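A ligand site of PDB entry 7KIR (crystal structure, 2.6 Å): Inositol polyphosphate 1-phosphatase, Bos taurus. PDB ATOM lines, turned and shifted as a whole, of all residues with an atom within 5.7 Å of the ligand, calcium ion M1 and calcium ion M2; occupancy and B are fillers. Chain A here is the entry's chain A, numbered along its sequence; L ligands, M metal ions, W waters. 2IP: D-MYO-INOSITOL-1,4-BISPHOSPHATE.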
ATOM      1  N   LYS A  50      12.818  34.061 -22.098  1.00  0.00           N
ATOM      2  CA  LYS A  50      13.410  32.746 -21.896  1.00  0.00           C
ATOM      3  C   LYS A  50      13.389  31.933 -23.188  1.00  0.00           C
ATOM      4  O   LYS A  50      14.411  31.346 -23.590  1.00  0.00           O
ATOM      5  CB  LYS A  50      12.718  32.011 -20.739  1.00  0.00           C
ATOM      6  CG  LYS A  50      11.265  31.559 -20.988  1.00  0.00           C
ATOM      7  CD  LYS A  50      11.014  30.142 -20.490  1.00  0.00           C
ATOM      8  CE  LYS A  50       9.833  29.481 -21.171  1.00  0.00           C
ATOM      9  NZ  LYS A  50      10.006  27.999 -21.200  1.00  0.00           N
ATOM     10  N   GLU A  79      14.344  20.919 -28.733  1.00  0.00           N
ATOM     11  CA  GLU A  79      13.098  21.245 -28.050  1.00  0.00           C
ATOM     12  C   GLU A  79      12.450  22.507 -28.609  1.00  0.00           C
ATOM     13  O   GLU A  79      11.220  22.631 -28.588  1.00  0.00           O
ATOM     14  CB  GLU A  79      13.350  21.400 -26.550  1.00  0.00           C
ATOM     15  CG  GLU A  79      12.098  21.658 -25.746  1.00  0.00           C
ATOM     16  CD  GLU A  79      12.406  21.956 -24.308  1.00  0.00           C
ATOM     17  OE1 GLU A  79      13.600  22.153 -23.999  1.00  0.00           O
ATOM     18  OE2 GLU A  79      11.461  21.991 -23.487  1.00  0.00           O
ATOM     19  N   GLU A  80      13.238  23.441 -29.115  1.00  0.00           N
ATOM     20  CA  GLU A  80      12.704  24.730 -29.522  1.00  0.00           C
ATOM     21  C   GLU A  80      12.431  24.763 -31.019  1.00  0.00           C
ATOM     22  O   GLU A  80      13.093  24.100 -31.824  1.00  0.00           O
ATOM     23  CB  GLU A  80      13.660  25.858 -29.138  1.00  0.00           C
ATOM     24  CG  GLU A  80      13.861  25.987 -27.642  1.00  0.00           C
ATOM     25  CD  GLU A  80      12.550  26.088 -26.890  1.00  0.00           C
ATOM     26  OE1 GLU A  80      11.642  26.803 -27.362  1.00  0.00           O
ATOM     27  OE2 GLU A  80      12.420  25.453 -25.831  1.00  0.00           O
ATOM     28  N   ASP A 153      18.834  20.030 -26.215  1.00  0.00           N
ATOM     29  CA  ASP A 153      18.140  20.923 -25.305  1.00  0.00           C
ATOM     30  C   ASP A 153      19.034  22.128 -25.073  1.00  0.00           C
ATOM     31  O   ASP A 153      20.067  21.998 -24.391  1.00  0.00           O
ATOM     32  CB  ASP A 153      17.813  20.229 -23.985  1.00  0.00           C
ATOM     33  CG  ASP A 153      16.815  21.018 -23.170  1.00  0.00           C
ATOM     34  OD1 ASP A 153      16.583  22.190 -23.499  1.00  0.00           O
ATOM     35  OD2 ASP A 153      16.253  20.462 -22.201  1.00  0.00           O
ATOM     36  N   PRO A 154      18.696  23.286 -25.628  1.00  0.00           N
ATOM     37  CA  PRO A 154      19.575  24.459 -25.479  1.00  0.00           C
ATOM     38  C   PRO A 154      19.754  24.896 -24.027  1.00  0.00           C
ATOM     39  O   PRO A 154      20.876  25.227 -23.628  1.00  0.00           O
ATOM     40  CB  PRO A 154      18.878  25.522 -26.328  1.00  0.00           C
ATOM     41  CG  PRO A 154      17.456  25.037 -26.465  1.00  0.00           C
ATOM     42  CD  PRO A 154      17.532  23.562 -26.476  1.00  0.00           C
ATOM     43  N   ILE A 155      18.685  24.924 -23.233  1.00  0.00           N
ATOM     44  CA  ILE A 155      18.772  25.279 -21.821  1.00  0.00           C
ATOM     45  C   ILE A 155      17.840  24.363 -21.041  1.00  0.00           C
ATOM     46  O   ILE A 155      16.612  24.491 -21.144  1.00  0.00           O
ATOM     47  CB  ILE A 155      18.409  26.751 -21.544  1.00  0.00           C
ATOM     48  CG1 ILE A 155      19.286  27.728 -22.325  1.00  0.00           C
ATOM     49  CG2 ILE A 155      18.474  27.026 -20.035  1.00  0.00           C
ATOM     50  CD1 ILE A 155      18.743  29.144 -22.346  1.00  0.00           C
ATOM     51  N   ASP A 156      18.414  23.460 -20.266  1.00  0.00           N
ATOM     52  CA  ASP A 156      17.616  22.575 -19.426  1.00  0.00           C
ATOM     53  C   ASP A 156      17.505  23.152 -18.019  1.00  0.00           C
ATOM     54  O   ASP A 156      18.440  23.786 -17.521  1.00  0.00           O
ATOM     55  CB  ASP A 156      18.226  21.180 -19.377  1.00  0.00           C
ATOM     56  CG  ASP A 156      17.342  20.190 -18.657  1.00  0.00           C
ATOM     57  OD1 ASP A 156      16.199  19.998 -19.107  1.00  0.00           O
ATOM     58  OD2 ASP A 156      17.766  19.604 -17.637  1.00  0.00           O
ATOM     59  N   SER A 157      16.347  22.920 -17.393  1.00  0.00           N
ATOM     60  CA  SER A 157      15.939  23.549 -16.134  1.00  0.00           C
ATOM     61  C   SER A 157      15.804  25.060 -16.311  1.00  0.00           C
ATOM     62  O   SER A 157      16.551  25.872 -15.766  1.00  0.00           O
ATOM     63  CB  SER A 157      16.901  23.208 -14.989  1.00  0.00           C
ATOM     64  OG  SER A 157      16.333  23.542 -13.739  1.00  0.00           O
ATOM     65  N   THR A 158      14.797  25.427 -17.119  1.00  0.00           N
ATOM     66  CA  THR A 158      14.579  26.823 -17.455  1.00  0.00           C
ATOM     67  C   THR A 158      14.116  27.620 -16.237  1.00  0.00           C
ATOM     68  O   THR A 158      14.447  28.819 -16.106  1.00  0.00           O
ATOM     69  CB  THR A 158      13.553  26.949 -18.592  1.00  0.00           C
ATOM     70  OG1 THR A 158      13.716  25.853 -19.492  1.00  0.00           O
ATOM     71  CG2 THR A 158      13.775  28.226 -19.354  1.00  0.00           C
ATOM     72  N   TYR A 159      13.377  26.989 -15.323  1.00  0.00           N
ATOM     73  CA  TYR A 159      12.871  27.692 -14.155  1.00  0.00           C
ATOM     74  C   TYR A 159      14.010  28.060 -13.198  1.00  0.00           C
ATOM     75  O   TYR A 159      13.979  29.113 -12.559  1.00  0.00           O
ATOM     76  CB  TYR A 159      11.814  26.847 -13.439  1.00  0.00           C
ATOM     77  CG  TYR A 159      11.308  27.480 -12.171  1.00  0.00           C
ATOM     78  CD1 TYR A 159      10.359  28.502 -12.206  1.00  0.00           C
ATOM     79  CD2 TYR A 159      11.772  27.064 -10.925  1.00  0.00           C
ATOM     80  CE1 TYR A 159       9.897  29.082 -11.051  1.00  0.00           C
ATOM     81  CE2 TYR A 159      11.318  27.641  -9.758  1.00  0.00           C
ATOM     82  CZ  TYR A 159      10.373  28.652  -9.833  1.00  0.00           C
ATOM     83  OH  TYR A 159       9.919  29.230  -8.667  1.00  0.00           O
ATOM     84  N   SER A 268      13.271  14.087  -9.008  1.00  0.00           N
ATOM     85  CA  SER A 268      12.997  15.461  -9.406  1.00  0.00           C
ATOM     86  C   SER A 268      12.186  16.170  -8.318  1.00  0.00           C
ATOM     87  O   SER A 268      11.851  15.595  -7.276  1.00  0.00           O
ATOM     88  CB  SER A 268      12.283  15.484 -10.750  1.00  0.00           C
ATOM     89  OG  SER A 268      10.880  15.644 -10.616  1.00  0.00           O
ATOM     90  N   GLU A 269      11.859  17.437  -8.559  1.00  0.00           N
ATOM     91  CA  GLU A 269      11.244  18.246  -7.529  1.00  0.00           C
ATOM     92  C   GLU A 269       9.759  17.986  -7.354  1.00  0.00           C
ATOM     93  O   GLU A 269       9.193  18.326  -6.308  1.00  0.00           O
ATOM     94  CB  GLU A 269      11.464  19.722  -7.851  1.00  0.00           C
ATOM     95  CG  GLU A 269      12.905  20.020  -8.128  1.00  0.00           C
ATOM     96  CD  GLU A 269      13.196  21.497  -8.070  1.00  0.00           C
ATOM     97  OE1 GLU A 269      12.308  22.298  -8.440  1.00  0.00           O
ATOM     98  OE2 GLU A 269      14.310  21.854  -7.616  1.00  0.00           O
ATOM     99  N   LYS A 270       9.105  17.408  -8.366  1.00  0.00           N
ATOM    100  CA  LYS A 270       7.673  17.165  -8.305  1.00  0.00           C
ATOM    101  C   LYS A 270       7.361  15.670  -8.352  1.00  0.00           C
ATOM    102  O   LYS A 270       6.231  15.284  -8.668  1.00  0.00           O
ATOM    103  CB  LYS A 270       6.960  17.898  -9.440  1.00  0.00           C
ATOM    104  CG  LYS A 270       7.392  17.446 -10.819  1.00  0.00           C
ATOM    105  CD  LYS A 270       8.516  18.309 -11.350  1.00  0.00           C
ATOM    106  CE  LYS A 270       8.498  18.397 -12.869  1.00  0.00           C
ATOM    107  NZ  LYS A 270       9.502  19.407 -13.301  1.00  0.00           N
ATOM    108  N   ALA A 288      16.399  17.160  -6.636  1.00  0.00           N
ATOM    109  CA  ALA A 288      17.230  18.066  -7.434  1.00  0.00           C
ATOM    110  C   ALA A 288      16.461  18.490  -8.673  1.00  0.00           C
ATOM    111  O   ALA A 288      15.627  17.747  -9.186  1.00  0.00           O
ATOM    112  CB  ALA A 288      18.556  17.415  -7.828  1.00  0.00           C
ATOM    113  N   ALA A 289      16.757  19.695  -9.142  1.00  0.00           N
ATOM    114  CA  ALA A 289      16.164  20.224 -10.361  1.00  0.00           C
ATOM    115  C   ALA A 289      17.035  19.884 -11.563  1.00  0.00           C
ATOM    116  O   ALA A 289      18.257  19.755 -11.447  1.00  0.00           O
ATOM    117  CB  ALA A 289      15.992  21.747 -10.262  1.00  0.00           C
ATOM    118  N   GLY A 290      16.382  19.711 -12.711  1.00  0.00           N
ATOM    119  CA  GLY A 290      17.103  19.468 -13.953  1.00  0.00           C
ATOM    120  C   GLY A 290      17.244  18.007 -14.334  1.00  0.00           C
ATOM    121  O   GLY A 290      17.764  17.196 -13.562  1.00  0.00           O
ATOM    122  N   ALA A 291      16.764  17.654 -15.537  1.00  0.00           N
ATOM    123  CA  ALA A 291      16.989  16.307 -16.058  1.00  0.00           C
ATOM    124  C   ALA A 291      18.457  16.089 -16.383  1.00  0.00           C
ATOM    125  O   ALA A 291      19.064  15.086 -15.987  1.00  0.00           O
ATOM    126  CB  ALA A 291      16.120  16.072 -17.286  1.00  0.00           C
ATOM    127  N   GLY A 292      19.049  17.053 -17.104  1.00  0.00           N
ATOM    128  CA  GLY A 292      20.471  16.986 -17.373  1.00  0.00           C
ATOM    129  C   GLY A 292      21.299  16.952 -16.103  1.00  0.00           C
ATOM    130  O   GLY A 292      22.227  16.146 -15.990  1.00  0.00           O
ATOM    131  N   LYS A 294      20.454  15.901 -13.045  1.00  0.00           N
ATOM    132  CA  LYS A 294      20.351  14.635 -12.313  1.00  0.00           C
ATOM    133  C   LYS A 294      21.113  13.528 -13.018  1.00  0.00           C
ATOM    134  O   LYS A 294      21.829  12.745 -12.370  1.00  0.00           O
ATOM    135  CB  LYS A 294      18.877  14.255 -12.127  1.00  0.00           C
ATOM    136  CG  LYS A 294      18.183  15.076 -11.038  1.00  0.00           C
ATOM    137  CD  LYS A 294      16.765  14.598 -10.745  1.00  0.00           C
ATOM    138  CE  LYS A 294      15.765  15.204 -11.711  1.00  0.00           C
ATOM    139  NZ  LYS A 294      15.846  16.695 -11.703  1.00  0.00           N
ATOM    140  N   TYR A 306      18.870   7.417 -10.959  1.00  0.00           N
ATOM    141  CA  TYR A 306      17.992   8.565 -11.194  1.00  0.00           C
ATOM    142  C   TYR A 306      16.690   8.009 -11.766  1.00  0.00           C
ATOM    143  O   TYR A 306      16.674   7.462 -12.874  1.00  0.00           O
ATOM    144  CB  TYR A 306      18.680   9.575 -12.115  1.00  0.00           C
ATOM    145  CG  TYR A 306      17.793  10.515 -12.906  1.00  0.00           C
ATOM    146  CD1 TYR A 306      16.689  11.135 -12.333  1.00  0.00           C
ATOM    147  CD2 TYR A 306      18.100  10.810 -14.225  1.00  0.00           C
ATOM    148  CE1 TYR A 306      15.889  11.990 -13.073  1.00  0.00           C
ATOM    149  CE2 TYR A 306      17.314  11.665 -14.965  1.00  0.00           C
ATOM    150  CZ  TYR A 306      16.216  12.261 -14.393  1.00  0.00           C
ATOM    151  OH  TYR A 306      15.444  13.116 -15.135  1.00  0.00           O
ATOM    152  N   PHE A 308      12.578   8.527 -12.772  1.00  0.00           N
ATOM    153  CA  PHE A 308      11.539   9.484 -13.144  1.00  0.00           C
ATOM    154  C   PHE A 308      10.318   8.697 -13.594  1.00  0.00           C
ATOM    155  O   PHE A 308      10.371   7.988 -14.598  1.00  0.00           O
ATOM    156  CB  PHE A 308      12.016  10.418 -14.238  1.00  0.00           C
ATOM    157  CG  PHE A 308      11.162  11.633 -14.397  1.00  0.00           C
ATOM    158  CD1 PHE A 308      10.191  11.689 -15.384  1.00  0.00           C
ATOM    159  CD2 PHE A 308      11.316  12.707 -13.532  1.00  0.00           C
ATOM    160  CE1 PHE A 308       9.400  12.815 -15.519  1.00  0.00           C
ATOM    161  CE2 PHE A 308      10.526  13.824 -13.652  1.00  0.00           C
ATOM    162  CZ  PHE A 308       9.576  13.886 -14.644  1.00  0.00           C
ATOM    163  N   THR A 312       7.100  13.215 -18.535  1.00  0.00           N
ATOM    164  CA  THR A 312       7.380  14.602 -18.866  1.00  0.00           C
ATOM    165  C   THR A 312       8.840  14.860 -19.226  1.00  0.00           C
ATOM    166  O   THR A 312       9.257  16.015 -19.307  1.00  0.00           O
ATOM    167  CB  THR A 312       6.928  15.506 -17.721  1.00  0.00           C
ATOM    168  OG1 THR A 312       7.453  15.000 -16.483  1.00  0.00           O
ATOM    169  CG2 THR A 312       5.409  15.522 -17.639  1.00  0.00           C
ATOM    170  N   THR A 313       9.619  13.809 -19.481  1.00  0.00           N
ATOM    171  CA  THR A 313      10.921  13.978 -20.127  1.00  0.00           C
ATOM    172  C   THR A 313      10.800  13.586 -21.584  1.00  0.00           C
ATOM    173  O   THR A 313       9.829  12.940 -22.006  1.00  0.00           O
ATOM    174  CB  THR A 313      12.029  13.158 -19.449  1.00  0.00           C
ATOM    175  OG1 THR A 313      11.848  11.762 -19.736  1.00  0.00           O
ATOM    176  CG2 THR A 313      12.042  13.386 -17.957  1.00  0.00           C
ATOM    177  N   PHE A 314      11.800  13.987 -22.362  1.00  0.00           N
ATOM    178  CA  PHE A 314      11.807  13.780 -23.810  1.00  0.00           C
ATOM    179  C   PHE A 314      13.217  13.385 -24.245  1.00  0.00           C
ATOM    180  O   PHE A 314      14.159  13.410 -23.448  1.00  0.00           O
ATOM    181  CB  PHE A 314      11.347  15.038 -24.566  1.00  0.00           C
ATOM    182  CG  PHE A 314      10.090  15.652 -24.018  1.00  0.00           C
ATOM    183  CD1 PHE A 314       8.861  15.381 -24.600  1.00  0.00           C
ATOM    184  CD2 PHE A 314      10.129  16.504 -22.925  1.00  0.00           C
ATOM    185  CE1 PHE A 314       7.697  15.941 -24.103  1.00  0.00           C
ATOM    186  CE2 PHE A 314       8.975  17.066 -22.408  1.00  0.00           C
ATOM    187  CZ  PHE A 314       7.759  16.791 -23.000  1.00  0.00           C
ATOM    188  N   TRP A 316      15.468  14.833 -26.011  1.00  0.00           N
ATOM    189  CA  TRP A 316      16.507  15.828 -25.828  1.00  0.00           C
ATOM    190  C   TRP A 316      16.920  15.992 -24.362  1.00  0.00           C
ATOM    191  O   TRP A 316      18.020  16.490 -24.107  1.00  0.00           O
ATOM    192  CB  TRP A 316      16.068  17.175 -26.395  1.00  0.00           C
ATOM    193  CG  TRP A 316      14.754  17.656 -25.878  1.00  0.00           C
ATOM    194  CD1 TRP A 316      14.525  18.326 -24.703  1.00  0.00           C
ATOM    195  CD2 TRP A 316      13.481  17.528 -26.523  1.00  0.00           C
ATOM    196  NE1 TRP A 316      13.183  18.612 -24.568  1.00  0.00           N
ATOM    197  CE2 TRP A 316      12.523  18.133 -25.670  1.00  0.00           C
ATOM    198  CE3 TRP A 316      13.050  16.955 -27.727  1.00  0.00           C
ATOM    199  CZ2 TRP A 316      11.165  18.189 -26.003  1.00  0.00           C
ATOM    200  CZ3 TRP A 316      11.694  17.003 -28.046  1.00  0.00           C
ATOM    201  CH2 TRP A 316      10.771  17.617 -27.190  1.00  0.00           C
ATOM    202  N   ASP A 317      16.071  15.601 -23.417  1.00  0.00           N
ATOM    203  CA  ASP A 317      16.468  15.640 -22.000  1.00  0.00           C
ATOM    204  C   ASP A 317      17.497  14.577 -21.688  1.00  0.00           C
ATOM    205  O   ASP A 317      18.380  14.797 -20.844  1.00  0.00           O
ATOM    206  CB  ASP A 317      15.252  15.445 -21.096  1.00  0.00           C
ATOM    207  CG  ASP A 317      14.394  16.687 -21.000  1.00  0.00           C
ATOM    208  OD1 ASP A 317      14.964  17.787 -21.016  1.00  0.00           O
ATOM    209  OD2 ASP A 317      13.156  16.561 -20.894  1.00  0.00           O
HETATM  210  C1  2IP L   1      12.245  20.186 -17.917  1.00  0.00           C
HETATM  211  C2  2IP L   1      13.547  20.037 -17.167  1.00  0.00           C
HETATM  212  C3  2IP L   1      13.089  19.763 -15.798  1.00  0.00           C
HETATM  213  C4  2IP L   1      12.353  18.475 -15.597  1.00  0.00           C
HETATM  214  C5  2IP L   1      11.127  18.530 -16.500  1.00  0.00           C
HETATM  215  C6  2IP L   1      11.597  18.824 -17.891  1.00  0.00           C
HETATM  216  O1  2IP L   1      12.573  20.684 -19.156  1.00  0.00           O
HETATM  217  O2  2IP L   1      14.253  18.906 -17.554  1.00  0.00           O
HETATM  218  O3  2IP L   1      14.285  19.769 -15.098  1.00  0.00           O
HETATM  219  O4  2IP L   1      11.816  18.493 -14.356  1.00  0.00           O
HETATM  220  O5  2IP L   1      10.452  17.318 -16.353  1.00  0.00           O
HETATM  221  O6  2IP L   1      10.433  18.875 -18.654  1.00  0.00           O
HETATM  222  P4  2IP L   1      12.739  18.347 -13.010  1.00  0.00           P
HETATM  223  O41 2IP L   1      13.813  17.320 -13.154  1.00  0.00           O
HETATM  224  O42 2IP L   1      11.650  18.217 -11.840  1.00  0.00           O
HETATM  225  O43 2IP L   1      13.424  19.775 -12.749  1.00  0.00           O
HETATM  226  P1  2IP L   1      12.795  22.278 -19.278  1.00  0.00           P
HETATM  227  O11 2IP L   1      13.829  22.376 -20.417  1.00  0.00           O
HETATM  228  O12 2IP L   1      13.495  22.869 -18.156  1.00  0.00           O
HETATM  229  O13 2IP L   1      11.444  23.012 -19.633  1.00  0.00           O
HETATM  230 CA    CA M   1      14.380  20.065 -20.651  1.00  0.00          CA
HETATM  231 CA    CA M   2      14.717  23.375 -22.310  1.00  0.00          CA
HETATM  232  O   HOH W   1      12.108  23.958 -16.218  1.00  0.00           O
HETATM  233  O   HOH W   2      11.662  19.488 -21.770  1.00  0.00           O
HETATM  234  O   HOH W   3      13.954  22.049 -14.006  1.00  0.00           O
HETATM  235  O   HOH W   4      12.202  24.365 -21.835  1.00  0.00           O
HETATM  236  O   HOH W   5      13.513  14.751 -14.051  1.00  0.00           O
HETATM  237  O   HOH W   6      14.454  25.445 -23.916  1.00  0.00           O
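Of the 26 residues printed, 3 come within 4 Å of calcium ion M1.
The side-chain carboxylate (OD2) of Asp 317 lies within hydrogen-bond range of the backbone NH (N) of Phe 314 (3.3 Å). The side-chain carboxylate (OD2) of Asp 156 lies within hydrogen-bond range of the backbone NH (N) of Ala 291, at 3.0 Å. The side-chain carboxylate of Asp 156 lies within hydrogen-bond range of the backbone NH of Gly 292. The backbone carbonyl oxygen (O) of Gly 290 sits at hydrogen-bond distance from the side-chain amino group (NZ) of Lys 294, at 2.7 Å. The backbone carbonyl oxygen (O) of Ala 288 is in hydrogen-bond range of the side-chain amino group (NZ) of Lys 294 (2.7 Å). OG of Ser 268 lies close to N of Lys 270, at 3.4 Å.
Calcium ion M1 is bound by OD1 of Asp 317 (2.4 Å), OD1 of Asp 156 (2.4 Å), O11 of the ligand (2.4 Å), O1 of the ligand (2.4 Å) and OD2 of Asp 153 (2.5 Å). Slightly farther from calcium ion M1 lies water W2 (3.0 Å).
Calcium ion M2 is bound by an oxygen (O11) of the ligand (2.3 Å), the side-chain carboxylate of Glu 79 (2.4 Å), the backbone carbonyl oxygen of Ile 155 (2.5 Å), the side-chain carboxylate of Asp 153 (2.5 Å), water W6 (2.6 Å) and water W4 (2.7 Å).
NZ of Lys 294 is in salt-bridge range of O41 of the ligand. The side-chain amino group (NZ) of Lys 270 is in salt-bridge range of an oxygen (O42) of the ligand (2.9 Å). The side-chain hydroxyl of Ser 268 is in hydrogen-bond range of an oxygen (O42) of the ligand, 3.0 Å away. The backbone NH (N) of Ser 157 lies within hydrogen-bond range of an oxygen (O12) of the ligand (3.0 Å). N of Gly 290 lies within hydrogen-bond range of O43 of the ligand (3.0 Å). An oxygen (O12) of the ligand sits at hydrogen-bond distance from the backbone NH (N) of Thr 158 (3.1 Å). The side-chain hydroxyl (OG1) of Thr 158 is in hydrogen-bond range of an oxygen (O12) of the ligand. O of Thr 312 sits at hydrogen-bond distance from O6 of the ligand (3.2 Å). The backbone NH (N) of Ala 291 is in hydrogen-bond range of an oxygen (O3) of the ligand, at 3.3 Å. N of Glu 269 sits at hydrogen-bond distance from O42 of the ligand (3.4 Å).
Merely in contact with calcium ion M2: Thr 158 (3.9 Å). Four residues have an atom within 4 Å of calcium ion M2: Glu 79, Asp 153, Ile 155 and Thr 158.
Water W2 lies within hydrogen-bond range of OE2 of Glu 79, NE1 of Trp 316, OD2 of Asp 317 and O6 of the ligand. Water W4 lies within hydrogen-bond range of O13 of the ligand, OE2 of Glu 79 and OG1 of Thr 158. Water W3 bridges O3 of the ligand (2.5 Å) and OG of Ser 157 (2.8 Å). Water W1 lies within hydrogen-bond range of an oxygen (O12) of the ligand (2.6 Å), the backbone NH of Thr 158 (3.2 Å) and the backbone NH of Tyr 159 (3.4 Å). Water W5 lies within hydrogen-bond range of an oxygen (O41) of the ligand and the side-chain hydroxyl of Tyr 306.
Ala 289 touches the ligand (CA to O43, 3.7 Å). CZ of Phe 308 touches O5 of the ligand (3.9 Å). Hydrophobic or aromatic side chains within 4 Å of the ligand: Ala 291 and Phe 308. Of the 26 residues printed, 16 come within 4 Å of the ligand.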
